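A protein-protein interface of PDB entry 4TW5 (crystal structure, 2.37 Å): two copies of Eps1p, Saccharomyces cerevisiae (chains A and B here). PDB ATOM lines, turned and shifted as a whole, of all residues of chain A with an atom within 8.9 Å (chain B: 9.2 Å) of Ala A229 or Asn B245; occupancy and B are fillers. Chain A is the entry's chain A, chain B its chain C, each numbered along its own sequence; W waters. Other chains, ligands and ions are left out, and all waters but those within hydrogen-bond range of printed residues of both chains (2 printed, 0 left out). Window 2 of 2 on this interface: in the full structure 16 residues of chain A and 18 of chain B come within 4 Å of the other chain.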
ATOM      1  N   PHE A 174      23.841  16.817 -27.555  1.00  0.00           N
ATOM      2  CA  PHE A 174      22.651  17.300 -26.858  1.00  0.00           C
ATOM      3  C   PHE A 174      22.221  16.351 -25.711  1.00  0.00           C
ATOM      4  O   PHE A 174      22.000  15.148 -25.914  1.00  0.00           O
ATOM      5  CB  PHE A 174      21.521  17.481 -27.865  1.00  0.00           C
ATOM      6  CG  PHE A 174      21.839  18.473 -28.977  1.00  0.00           C
ATOM      7  CD1 PHE A 174      21.779  19.834 -28.752  1.00  0.00           C
ATOM      8  CD2 PHE A 174      22.186  18.030 -30.254  1.00  0.00           C
ATOM      9  CE1 PHE A 174      22.064  20.738 -29.774  1.00  0.00           C
ATOM     10  CE2 PHE A 174      22.456  18.933 -31.286  1.00  0.00           C
ATOM     11  CZ  PHE A 174      22.396  20.283 -31.038  1.00  0.00           C
ATOM     12  N   LYS A 175      22.039  16.910 -24.522  1.00  0.00           N
ATOM     13  CA  LYS A 175      21.592  16.130 -23.368  1.00  0.00           C
ATOM     14  C   LYS A 175      20.055  16.003 -23.311  1.00  0.00           C
ATOM     15  O   LYS A 175      19.321  16.980 -23.528  1.00  0.00           O
ATOM     16  CB  LYS A 175      22.114  16.774 -22.087  1.00  0.00           C
ATOM     17  CG  LYS A 175      23.621  16.976 -22.056  1.00  0.00           C
ATOM     18  CD  LYS A 175      24.346  15.649 -22.280  1.00  0.00           C
ATOM     19  CE  LYS A 175      25.847  15.864 -22.451  1.00  0.00           C
ATOM     20  NZ  LYS A 175      26.376  14.736 -23.275  1.00  0.00           N
ATOM     21  N   ASN A 176      19.577  14.793 -23.039  1.00  0.00           N
ATOM     22  CA  ASN A 176      18.143  14.523 -22.941  1.00  0.00           C
ATOM     23  C   ASN A 176      17.342  15.094 -24.142  1.00  0.00           C
ATOM     24  O   ASN A 176      16.252  15.666 -23.985  1.00  0.00           O
ATOM     25  CB  ASN A 176      17.610  15.067 -21.613  1.00  0.00           C
ATOM     26  CG  ASN A 176      18.353  14.497 -20.426  1.00  0.00           C
ATOM     27  OD1 ASN A 176      18.943  13.427 -20.533  1.00  0.00           O
ATOM     28  ND2 ASN A 176      18.338  15.203 -19.295  1.00  0.00           N
ATOM     29  N   CYS A 177      17.905  14.935 -25.334  1.00  0.00           N
ATOM     30  CA  CYS A 177      17.243  15.353 -26.551  1.00  0.00           C
ATOM     31  C   CYS A 177      17.529  14.378 -27.665  1.00  0.00           C
ATOM     32  O   CYS A 177      18.439  14.591 -28.457  1.00  0.00           O
ATOM     33  CB  CYS A 177      17.688  16.757 -26.976  1.00  0.00           C
ATOM     34  SG  CYS A 177      16.796  17.390 -28.433  1.00  0.00           S
ATOM     35  N   ASP A 178      16.712  13.334 -27.742  1.00  0.00           N
ATOM     36  CA  ASP A 178      16.872  12.279 -28.726  1.00  0.00           C
ATOM     37  C   ASP A 178      16.790  12.780 -30.165  1.00  0.00           C
ATOM     38  O   ASP A 178      17.462  12.256 -31.046  1.00  0.00           O
ATOM     39  CB  ASP A 178      15.810  11.201 -28.520  1.00  0.00           C
ATOM     40  CG  ASP A 178      15.965  10.459 -27.200  1.00  0.00           C
ATOM     41  OD1 ASP A 178      17.097  10.394 -26.652  1.00  0.00           O
ATOM     42  OD2 ASP A 178      14.930   9.961 -26.701  1.00  0.00           O
ATOM     43  N   ILE A 224      18.774  21.035 -17.647  1.00  0.00           N
ATOM     44  CA  ILE A 224      18.616  19.598 -17.375  1.00  0.00           C
ATOM     45  C   ILE A 224      17.644  19.378 -16.199  1.00  0.00           C
ATOM     46  O   ILE A 224      17.777  20.046 -15.185  1.00  0.00           O
ATOM     47  CB  ILE A 224      19.981  18.931 -16.979  1.00  0.00           C
ATOM     48  CG1 ILE A 224      21.021  18.975 -18.099  1.00  0.00           C
ATOM     49  CG2 ILE A 224      19.766  17.496 -16.525  1.00  0.00           C
ATOM     50  CD1 ILE A 224      20.657  18.120 -19.284  1.00  0.00           C
ATOM     51  N   THR A 225      16.641  18.515 -16.341  1.00  0.00           N
ATOM     52  CA  THR A 225      15.857  18.048 -15.178  1.00  0.00           C
ATOM     53  C   THR A 225      15.593  16.550 -15.353  1.00  0.00           C
ATOM     54  O   THR A 225      15.383  16.102 -16.477  1.00  0.00           O
ATOM     55  CB  THR A 225      14.491  18.783 -15.009  1.00  0.00           C
ATOM     56  OG1 THR A 225      13.648  18.537 -16.139  1.00  0.00           O
ATOM     57  CG2 THR A 225      14.668  20.285 -14.807  1.00  0.00           C
ATOM     58  N   ASN A 226      15.541  15.767 -14.277  1.00  0.00           N
ATOM     59  CA  ASN A 226      15.320  14.331 -14.481  1.00  0.00           C
ATOM     60  C   ASN A 226      13.832  13.886 -14.454  1.00  0.00           C
ATOM     61  O   ASN A 226      13.524  12.690 -14.543  1.00  0.00           O
ATOM     62  CB  ASN A 226      16.164  13.508 -13.492  1.00  0.00           C
ATOM     63  CG  ASN A 226      17.664  13.859 -13.560  1.00  0.00           C
ATOM     64  OD1 ASN A 226      18.256  14.335 -12.584  1.00  0.00           O
ATOM     65  ND2 ASN A 226      18.279  13.620 -14.723  1.00  0.00           N
ATOM     66  N   HIS A 227      12.918  14.845 -14.330  1.00  0.00           N
ATOM     67  CA  HIS A 227      11.485  14.574 -14.505  1.00  0.00           C
ATOM     68  C   HIS A 227      11.095  14.489 -15.974  1.00  0.00           C
ATOM     69  O   HIS A 227      10.317  13.622 -16.350  1.00  0.00           O
ATOM     70  CB  HIS A 227      10.653  15.595 -13.747  1.00  0.00           C
ATOM     71  CG  HIS A 227      10.953  15.593 -12.285  1.00  0.00           C
ATOM     72  ND1 HIS A 227      11.627  16.619 -11.655  1.00  0.00           N
ATOM     73  CD2 HIS A 227      10.745  14.643 -11.341  1.00  0.00           C
ATOM     74  CE1 HIS A 227      11.773  16.322 -10.375  1.00  0.00           C
ATOM     75  NE2 HIS A 227      11.255  15.126 -10.162  1.00  0.00           N
ATOM     76  N   ARG A 228      11.623  15.363 -16.822  1.00  0.00           N
ATOM     77  CA  ARG A 228      11.359  15.161 -18.245  1.00  0.00           C
ATOM     78  C   ARG A 228      12.495  14.359 -18.832  1.00  0.00           C
ATOM     79  O   ARG A 228      13.655  14.788 -18.814  1.00  0.00           O
ATOM     80  CB  ARG A 228      11.197  16.474 -19.011  1.00  0.00           C
ATOM     81  CG  ARG A 228       9.947  17.241 -18.661  1.00  0.00           C
ATOM     82  CD  ARG A 228       9.835  18.461 -19.548  1.00  0.00           C
ATOM     83  NE  ARG A 228       8.622  19.213 -19.257  1.00  0.00           N
ATOM     84  CZ  ARG A 228       7.414  18.854 -19.659  1.00  0.00           C
ATOM     85  NH1 ARG A 228       7.242  17.737 -20.355  1.00  0.00           N
ATOM     86  NH2 ARG A 228       6.384  19.605 -19.340  1.00  0.00           N
ATOM     87  N   ALA A 229      12.130  13.202 -19.375  1.00  0.00           N
ATOM     88  CA  ALA A 229      13.063  12.270 -19.995  1.00  0.00           C
ATOM     89  C   ALA A 229      13.741  12.890 -21.207  1.00  0.00           C
ATOM     90  O   ALA A 229      14.945  12.726 -21.440  1.00  0.00           O
ATOM     91  CB  ALA A 229      12.330  10.983 -20.404  1.00  0.00           C
ATOM     92  N   ASP A 230      12.943  13.627 -21.961  1.00  0.00           N
ATOM     93  CA  ASP A 230      13.308  14.029 -23.292  1.00  0.00           C
ATOM     94  C   ASP A 230      12.729  15.397 -23.621  1.00  0.00           C
ATOM     95  O   ASP A 230      11.638  15.756 -23.171  1.00  0.00           O
ATOM     96  CB  ASP A 230      12.812  12.973 -24.276  1.00  0.00           C
ATOM     97  CG  ASP A 230      13.333  13.184 -25.679  1.00  0.00           C
ATOM     98  OD1 ASP A 230      14.559  13.092 -25.896  1.00  0.00           O
ATOM     99  OD2 ASP A 230      12.496  13.428 -26.570  1.00  0.00           O
ATOM    100  N   ARG A 231      13.492  16.150 -24.400  1.00  0.00           N
ATOM    101  CA  ARG A 231      13.117  17.468 -24.869  1.00  0.00           C
ATOM    102  C   ARG A 231      13.314  17.502 -26.378  1.00  0.00           C
ATOM    103  O   ARG A 231      14.098  16.717 -26.934  1.00  0.00           O
ATOM    104  CB  ARG A 231      13.966  18.542 -24.195  1.00  0.00           C
ATOM    105  CG  ARG A 231      14.354  18.174 -22.785  1.00  0.00           C
ATOM    106  CD  ARG A 231      15.309  19.166 -22.202  1.00  0.00           C
ATOM    107  NE  ARG A 231      16.695  18.885 -22.543  1.00  0.00           N
ATOM    108  CZ  ARG A 231      17.694  19.641 -22.124  1.00  0.00           C
ATOM    109  NH1 ARG A 231      17.437  20.700 -21.370  1.00  0.00           N
ATOM    110  NH2 ARG A 231      18.934  19.347 -22.450  1.00  0.00           N
ATOM    111  N   GLU A 232      12.660  18.459 -27.020  1.00  0.00           N
ATOM    112  CA  GLU A 232      12.747  18.650 -28.463  1.00  0.00           C
ATOM    113  C   GLU A 232      13.082  20.082 -28.773  1.00  0.00           C
ATOM    114  O   GLU A 232      12.702  20.975 -28.025  1.00  0.00           O
ATOM    115  CB  GLU A 232      11.415  18.363 -29.148  1.00  0.00           C
ATOM    116  CG  GLU A 232      10.993  16.945 -29.325  1.00  0.00           C
ATOM    117  CD  GLU A 232       9.638  16.897 -29.993  1.00  0.00           C
ATOM    118  OE1 GLU A 232       9.030  17.989 -30.104  1.00  0.00           O
ATOM    119  OE2 GLU A 232       9.193  15.797 -30.414  1.00  0.00           O
ATOM    120  N   ILE B 147       5.560  14.965  -8.494  1.00  0.00           N
ATOM    121  CA  ILE B 147       6.625  14.751  -9.445  1.00  0.00           C
ATOM    122  C   ILE B 147       7.897  14.194  -8.749  1.00  0.00           C
ATOM    123  O   ILE B 147       8.770  13.639  -9.410  1.00  0.00           O
ATOM    124  CB  ILE B 147       6.907  16.075 -10.216  1.00  0.00           C
ATOM    125  CG1 ILE B 147       6.894  15.828 -11.703  1.00  0.00           C
ATOM    126  CG2 ILE B 147       8.203  16.738  -9.805  1.00  0.00           C
ATOM    127  CD1 ILE B 147       5.568  15.447 -12.206  1.00  0.00           C
ATOM    128  N   ALA B 148       7.966  14.327  -7.422  1.00  0.00           N
ATOM    129  CA  ALA B 148       8.999  13.692  -6.591  1.00  0.00           C
ATOM    130  C   ALA B 148       8.753  12.191  -6.366  1.00  0.00           C
ATOM    131  O   ALA B 148       9.600  11.491  -5.808  1.00  0.00           O
ATOM    132  CB  ALA B 148       9.107  14.399  -5.257  1.00  0.00           C
ATOM    133  N   GLY B 149       7.603  11.708  -6.823  1.00  0.00           N
ATOM    134  CA  GLY B 149       7.278  10.295  -6.799  1.00  0.00           C
ATOM    135  C   GLY B 149       6.224   9.909  -5.782  1.00  0.00           C
ATOM    136  O   GLY B 149       6.049   8.733  -5.468  1.00  0.00           O
ATOM    137  N   LEU B 237       1.056  14.459 -18.076  1.00  0.00           N
ATOM    138  CA  LEU B 237       0.835  13.247 -17.301  1.00  0.00           C
ATOM    139  C   LEU B 237       1.957  12.966 -16.302  1.00  0.00           C
ATOM    140  O   LEU B 237       3.126  12.950 -16.671  1.00  0.00           O
ATOM    141  CB  LEU B 237       0.681  12.055 -18.240  1.00  0.00           C
ATOM    142  CG  LEU B 237       0.399  10.719 -17.559  1.00  0.00           C
ATOM    143  CD1 LEU B 237      -0.900  10.804 -16.788  1.00  0.00           C
ATOM    144  CD2 LEU B 237       0.326   9.586 -18.576  1.00  0.00           C
ATOM    145  N   VAL B 238       1.586  12.681 -15.051  1.00  0.00           N
ATOM    146  CA  VAL B 238       2.544  12.279 -14.027  1.00  0.00           C
ATOM    147  C   VAL B 238       2.425  10.787 -13.764  1.00  0.00           C
ATOM    148  O   VAL B 238       1.339  10.302 -13.442  1.00  0.00           O
ATOM    149  CB  VAL B 238       2.317  12.997 -12.690  1.00  0.00           C
ATOM    150  CG1 VAL B 238       3.479  12.705 -11.752  1.00  0.00           C
ATOM    151  CG2 VAL B 238       2.159  14.489 -12.889  1.00  0.00           C
ATOM    152  N   LEU B 239       3.517  10.041 -13.904  1.00  0.00           N
ATOM    153  CA  LEU B 239       3.431   8.617 -13.617  1.00  0.00           C
ATOM    154  C   LEU B 239       3.497   8.346 -12.101  1.00  0.00           C
ATOM    155  O   LEU B 239       4.172   9.044 -11.353  1.00  0.00           O
ATOM    156  CB  LEU B 239       4.511   7.852 -14.367  1.00  0.00           C
ATOM    157  CG  LEU B 239       4.352   7.923 -15.891  1.00  0.00           C
ATOM    158  CD1 LEU B 239       5.367   7.016 -16.567  1.00  0.00           C
ATOM    159  CD2 LEU B 239       2.921   7.589 -16.333  1.00  0.00           C
ATOM    160  N   PRO B 240       2.721   7.376 -11.630  1.00  0.00           N
ATOM    161  CA  PRO B 240       2.746   7.167 -10.170  1.00  0.00           C
ATOM    162  C   PRO B 240       4.033   6.459  -9.651  1.00  0.00           C
ATOM    163  O   PRO B 240       4.612   5.624 -10.332  1.00  0.00           O
ATOM    164  CB  PRO B 240       1.510   6.285  -9.925  1.00  0.00           C
ATOM    165  CG  PRO B 240       1.375   5.483 -11.187  1.00  0.00           C
ATOM    166  CD  PRO B 240       1.827   6.431 -12.328  1.00  0.00           C
ATOM    167  N   ASN B 241       4.475   6.849  -8.462  1.00  0.00           N
ATOM    168  CA  ASN B 241       5.532   6.156  -7.750  1.00  0.00           C
ATOM    169  C   ASN B 241       6.895   6.026  -8.485  1.00  0.00           C
ATOM    170  O   ASN B 241       7.651   5.119  -8.182  1.00  0.00           O
ATOM    171  CB  ASN B 241       5.010   4.769  -7.329  1.00  0.00           C
ATOM    172  CG  ASN B 241       3.954   4.853  -6.226  1.00  0.00           C
ATOM    173  OD1 ASN B 241       4.165   5.504  -5.196  1.00  0.00           O
ATOM    174  ND2 ASN B 241       2.796   4.228  -6.455  1.00  0.00           N
ATOM    175  N   LYS B 242       7.173   6.921  -9.440  1.00  0.00           N
ATOM    176  CA  LYS B 242       8.470   7.017 -10.122  1.00  0.00           C
ATOM    177  C   LYS B 242       9.110   8.327  -9.712  1.00  0.00           C
ATOM    178  O   LYS B 242       8.409   9.332  -9.586  1.00  0.00           O
ATOM    179  CB  LYS B 242       8.327   7.000 -11.647  1.00  0.00           C
ATOM    180  CG  LYS B 242       8.021   5.655 -12.246  1.00  0.00           C
ATOM    181  CD  LYS B 242       7.681   5.792 -13.724  1.00  0.00           C
ATOM    182  CE  LYS B 242       7.055   4.511 -14.270  1.00  0.00           C
ATOM    183  NZ  LYS B 242       7.764   3.284 -13.765  1.00  0.00           N
ATOM    184  N   THR B 243      10.419   8.341  -9.495  1.00  0.00           N
ATOM    185  CA  THR B 243      11.096   9.575  -9.066  1.00  0.00           C
ATOM    186  C   THR B 243      11.753  10.352 -10.218  1.00  0.00           C
ATOM    187  O   THR B 243      12.317  11.418 -10.014  1.00  0.00           O
ATOM    188  CB  THR B 243      12.181   9.292  -8.054  1.00  0.00           C
ATOM    189  OG1 THR B 243      13.076   8.313  -8.607  1.00  0.00           O
ATOM    190  CG2 THR B 243      11.559   8.811  -6.713  1.00  0.00           C
ATOM    191  N   SER B 244      11.720   9.768 -11.406  1.00  0.00           N
ATOM    192  CA  SER B 244      12.395  10.305 -12.565  1.00  0.00           C
ATOM    193  C   SER B 244      11.643   9.876 -13.790  1.00  0.00           C
ATOM    194  O   SER B 244      10.967   8.843 -13.762  1.00  0.00           O
ATOM    195  CB  SER B 244      13.836   9.803 -12.650  1.00  0.00           C
ATOM    196  OG  SER B 244      14.659  10.486 -11.726  1.00  0.00           O
ATOM    197  N   ASN B 245      11.792  10.655 -14.862  1.00  0.00           N
ATOM    198  CA  ASN B 245      11.107  10.386 -16.120  1.00  0.00           C
ATOM    199  C   ASN B 245       9.642  10.047 -15.872  1.00  0.00           C
ATOM    200  O   ASN B 245       9.111   9.068 -16.396  1.00  0.00           O
ATOM    201  CB  ASN B 245      11.790   9.249 -16.888  1.00  0.00           C
ATOM    202  CG  ASN B 245      13.244   9.569 -17.265  1.00  0.00           C
ATOM    203  OD1 ASN B 245      13.780  10.644 -16.950  1.00  0.00           O
ATOM    204  ND2 ASN B 245      13.881   8.628 -17.959  1.00  0.00           N
ATOM    205  N   ASN B 246       8.997  10.870 -15.057  1.00  0.00           N
ATOM    206  CA  ASN B 246       7.637  10.600 -14.657  1.00  0.00           C
ATOM    207  C   ASN B 246       6.674  11.663 -15.213  1.00  0.00           C
ATOM    208  O   ASN B 246       5.476  11.637 -14.915  1.00  0.00           O
ATOM    209  CB  ASN B 246       7.563  10.538 -13.131  1.00  0.00           C
ATOM    210  CG  ASN B 246       8.316  11.667 -12.493  1.00  0.00           C
ATOM    211  OD1 ASN B 246       8.789  12.563 -13.197  1.00  0.00           O
ATOM    212  ND2 ASN B 246       8.400  11.670 -11.168  1.00  0.00           N
ATOM    213  N   LEU B 247       7.204  12.597 -16.002  1.00  0.00           N
ATOM    214  CA  LEU B 247       6.384  13.697 -16.536  1.00  0.00           C
ATOM    215  C   LEU B 247       6.399  13.733 -18.052  1.00  0.00           C
ATOM    216  O   LEU B 247       7.409  13.993 -18.658  1.00  0.00           O
ATOM    217  CB  LEU B 247       6.843  15.046 -15.977  1.00  0.00           C
ATOM    218  CG  LEU B 247       5.970  16.253 -16.348  1.00  0.00           C
ATOM    219  CD1 LEU B 247       4.585  16.147 -15.799  1.00  0.00           C
ATOM    220  CD2 LEU B 247       6.606  17.496 -15.771  1.00  0.00           C
ATOM    221  N   PHE B 248       5.234  13.526 -18.638  1.00  0.00           N
ATOM    222  CA  PHE B 248       5.082  13.441 -20.073  1.00  0.00           C
ATOM    223  C   PHE B 248       3.982  14.393 -20.590  1.00  0.00           C
ATOM    224  O   PHE B 248       2.807  14.240 -20.236  1.00  0.00           O
ATOM    225  CB  PHE B 248       4.754  12.000 -20.458  1.00  0.00           C
ATOM    226  CG  PHE B 248       5.825  11.025 -20.092  1.00  0.00           C
ATOM    227  CD1 PHE B 248       6.899  10.794 -20.948  1.00  0.00           C
ATOM    228  CD2 PHE B 248       5.769  10.337 -18.889  1.00  0.00           C
ATOM    229  CE1 PHE B 248       7.890   9.898 -20.617  1.00  0.00           C
ATOM    230  CE2 PHE B 248       6.747   9.456 -18.554  1.00  0.00           C
ATOM    231  CZ  PHE B 248       7.807   9.229 -19.422  1.00  0.00           C
ATOM    232  N   ASP B 249       4.373  15.373 -21.404  1.00  0.00           N
ATOM    233  CA  ASP B 249       3.409  16.292 -22.037  1.00  0.00           C
ATOM    234  C   ASP B 249       2.453  15.583 -22.995  1.00  0.00           C
ATOM    235  O   ASP B 249       2.859  14.652 -23.698  1.00  0.00           O
ATOM    236  CB  ASP B 249       4.151  17.407 -22.800  1.00  0.00           C
ATOM    237  CG  ASP B 249       4.683  18.498 -21.882  1.00  0.00           C
ATOM    238  OD1 ASP B 249       4.450  18.415 -20.655  1.00  0.00           O
ATOM    239  OD2 ASP B 249       5.354  19.435 -22.377  1.00  0.00           O
ATOM    240  N   PHE B 269       3.167   3.013 -19.999  1.00  0.00           N
ATOM    241  CA  PHE B 269       4.499   3.622 -20.085  1.00  0.00           C
ATOM    242  C   PHE B 269       5.569   2.749 -19.413  1.00  0.00           C
ATOM    243  O   PHE B 269       5.722   2.758 -18.187  1.00  0.00           O
ATOM    244  CB  PHE B 269       4.494   5.015 -19.445  1.00  0.00           C
ATOM    245  CG  PHE B 269       3.626   6.023 -20.164  1.00  0.00           C
ATOM    246  CD1 PHE B 269       4.132   6.787 -21.214  1.00  0.00           C
ATOM    247  CD2 PHE B 269       2.293   6.188 -19.806  1.00  0.00           C
ATOM    248  CE1 PHE B 269       3.325   7.713 -21.868  1.00  0.00           C
ATOM    249  CE2 PHE B 269       1.486   7.099 -20.467  1.00  0.00           C
ATOM    250  CZ  PHE B 269       1.998   7.862 -21.490  1.00  0.00           C
HETATM  251  O   HOH W   1      13.676  13.941 -10.631  1.00  0.00           O
HETATM  252  O   HOH W   2       9.277  11.877 -18.904  1.00  0.00           O
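A ring nitrogen (NE2) of His A227 lies close to the backbone carbonyl oxygen (O) of Ile B147. O of Asn A226 is in hydrogen-bond range of N of Asn B245, 2.7 Å away. The guanidinium group (NH2) of Arg A228 is in salt-bridge range of the side-chain carboxylate (OD1) of Asp B249 (2.6 Å). O of His A227 is in hydrogen-bond range of N of Leu B247 (3.3 Å). The backbone carbonyl oxygen of His A227 is in hydrogen-bond range of the backbone NH of Asn B246 (3.3 Å).
Ala A229 touches just one residue of chain B: Asn B245 (3.5 Å). Of the printed residues of chain A, Ile B147 touches His A227. Of the printed residues of chain B, Arg A228 touches Asp B249. Printed residues of chain B within 4 Å of His A227: Ile B147 (2.9 Å), Thr B243 (3.8 Å), Asn B245 (3.3 Å), Asn B246 (3.3 Å) and Leu B247 (3.3 Å). Of the printed residues of chain A, Thr B243 touches His A227 (3.8 Å). Val B238 touches none of the printed residues of chain A. Asn A176 touches none of the printed residues of chain B.
O of Asn B246 sits at hydrogen-bond distance from N of Leu B239 (2.7 Å). O of Ile B147 lies within hydrogen-bond range of ND2 of Asn B246 (2.7 Å). The backbone carbonyl oxygen (O) of Lys B242 lies within hydrogen-bond range of the side-chain amide nitrogen (ND2) of Asn B246, at 2.8 Å.
No position is printed for both chains. Of the 9 pairs that touch across the chains among the printed residues, none has its exchanged pair printed and touching as well.
Of the 14 printed residues of chain A, 4 touch a printed residue of chain B. Printed residues of chain B that touch a printed residue of chain A: Ile B147, Thr B243, Ser B244, Asn B245, Asn B246, Leu B247 and Asp B249. Among the printed residues, 9 pairs touch across the chains. Among the printed residues, Asp or Glu carboxylates within 4 Å of a Lys or Arg side-chain nitrogen of the other chain: Arg A228 with Asp B249 (2.6 Å).
Among the printed residues, pairs that only touch across the chains: Asn A226 with Ser B244, His A227 with Asn B245, Ala A229 with Asn B245 and His A227 with Thr B243.
Water W1 lies within hydrogen-bond range of NE2 of His A227 and O of Thr B243. Water W2 lies within hydrogen-bond range of O of Leu B247, N of Ala A229 and O of His A227.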
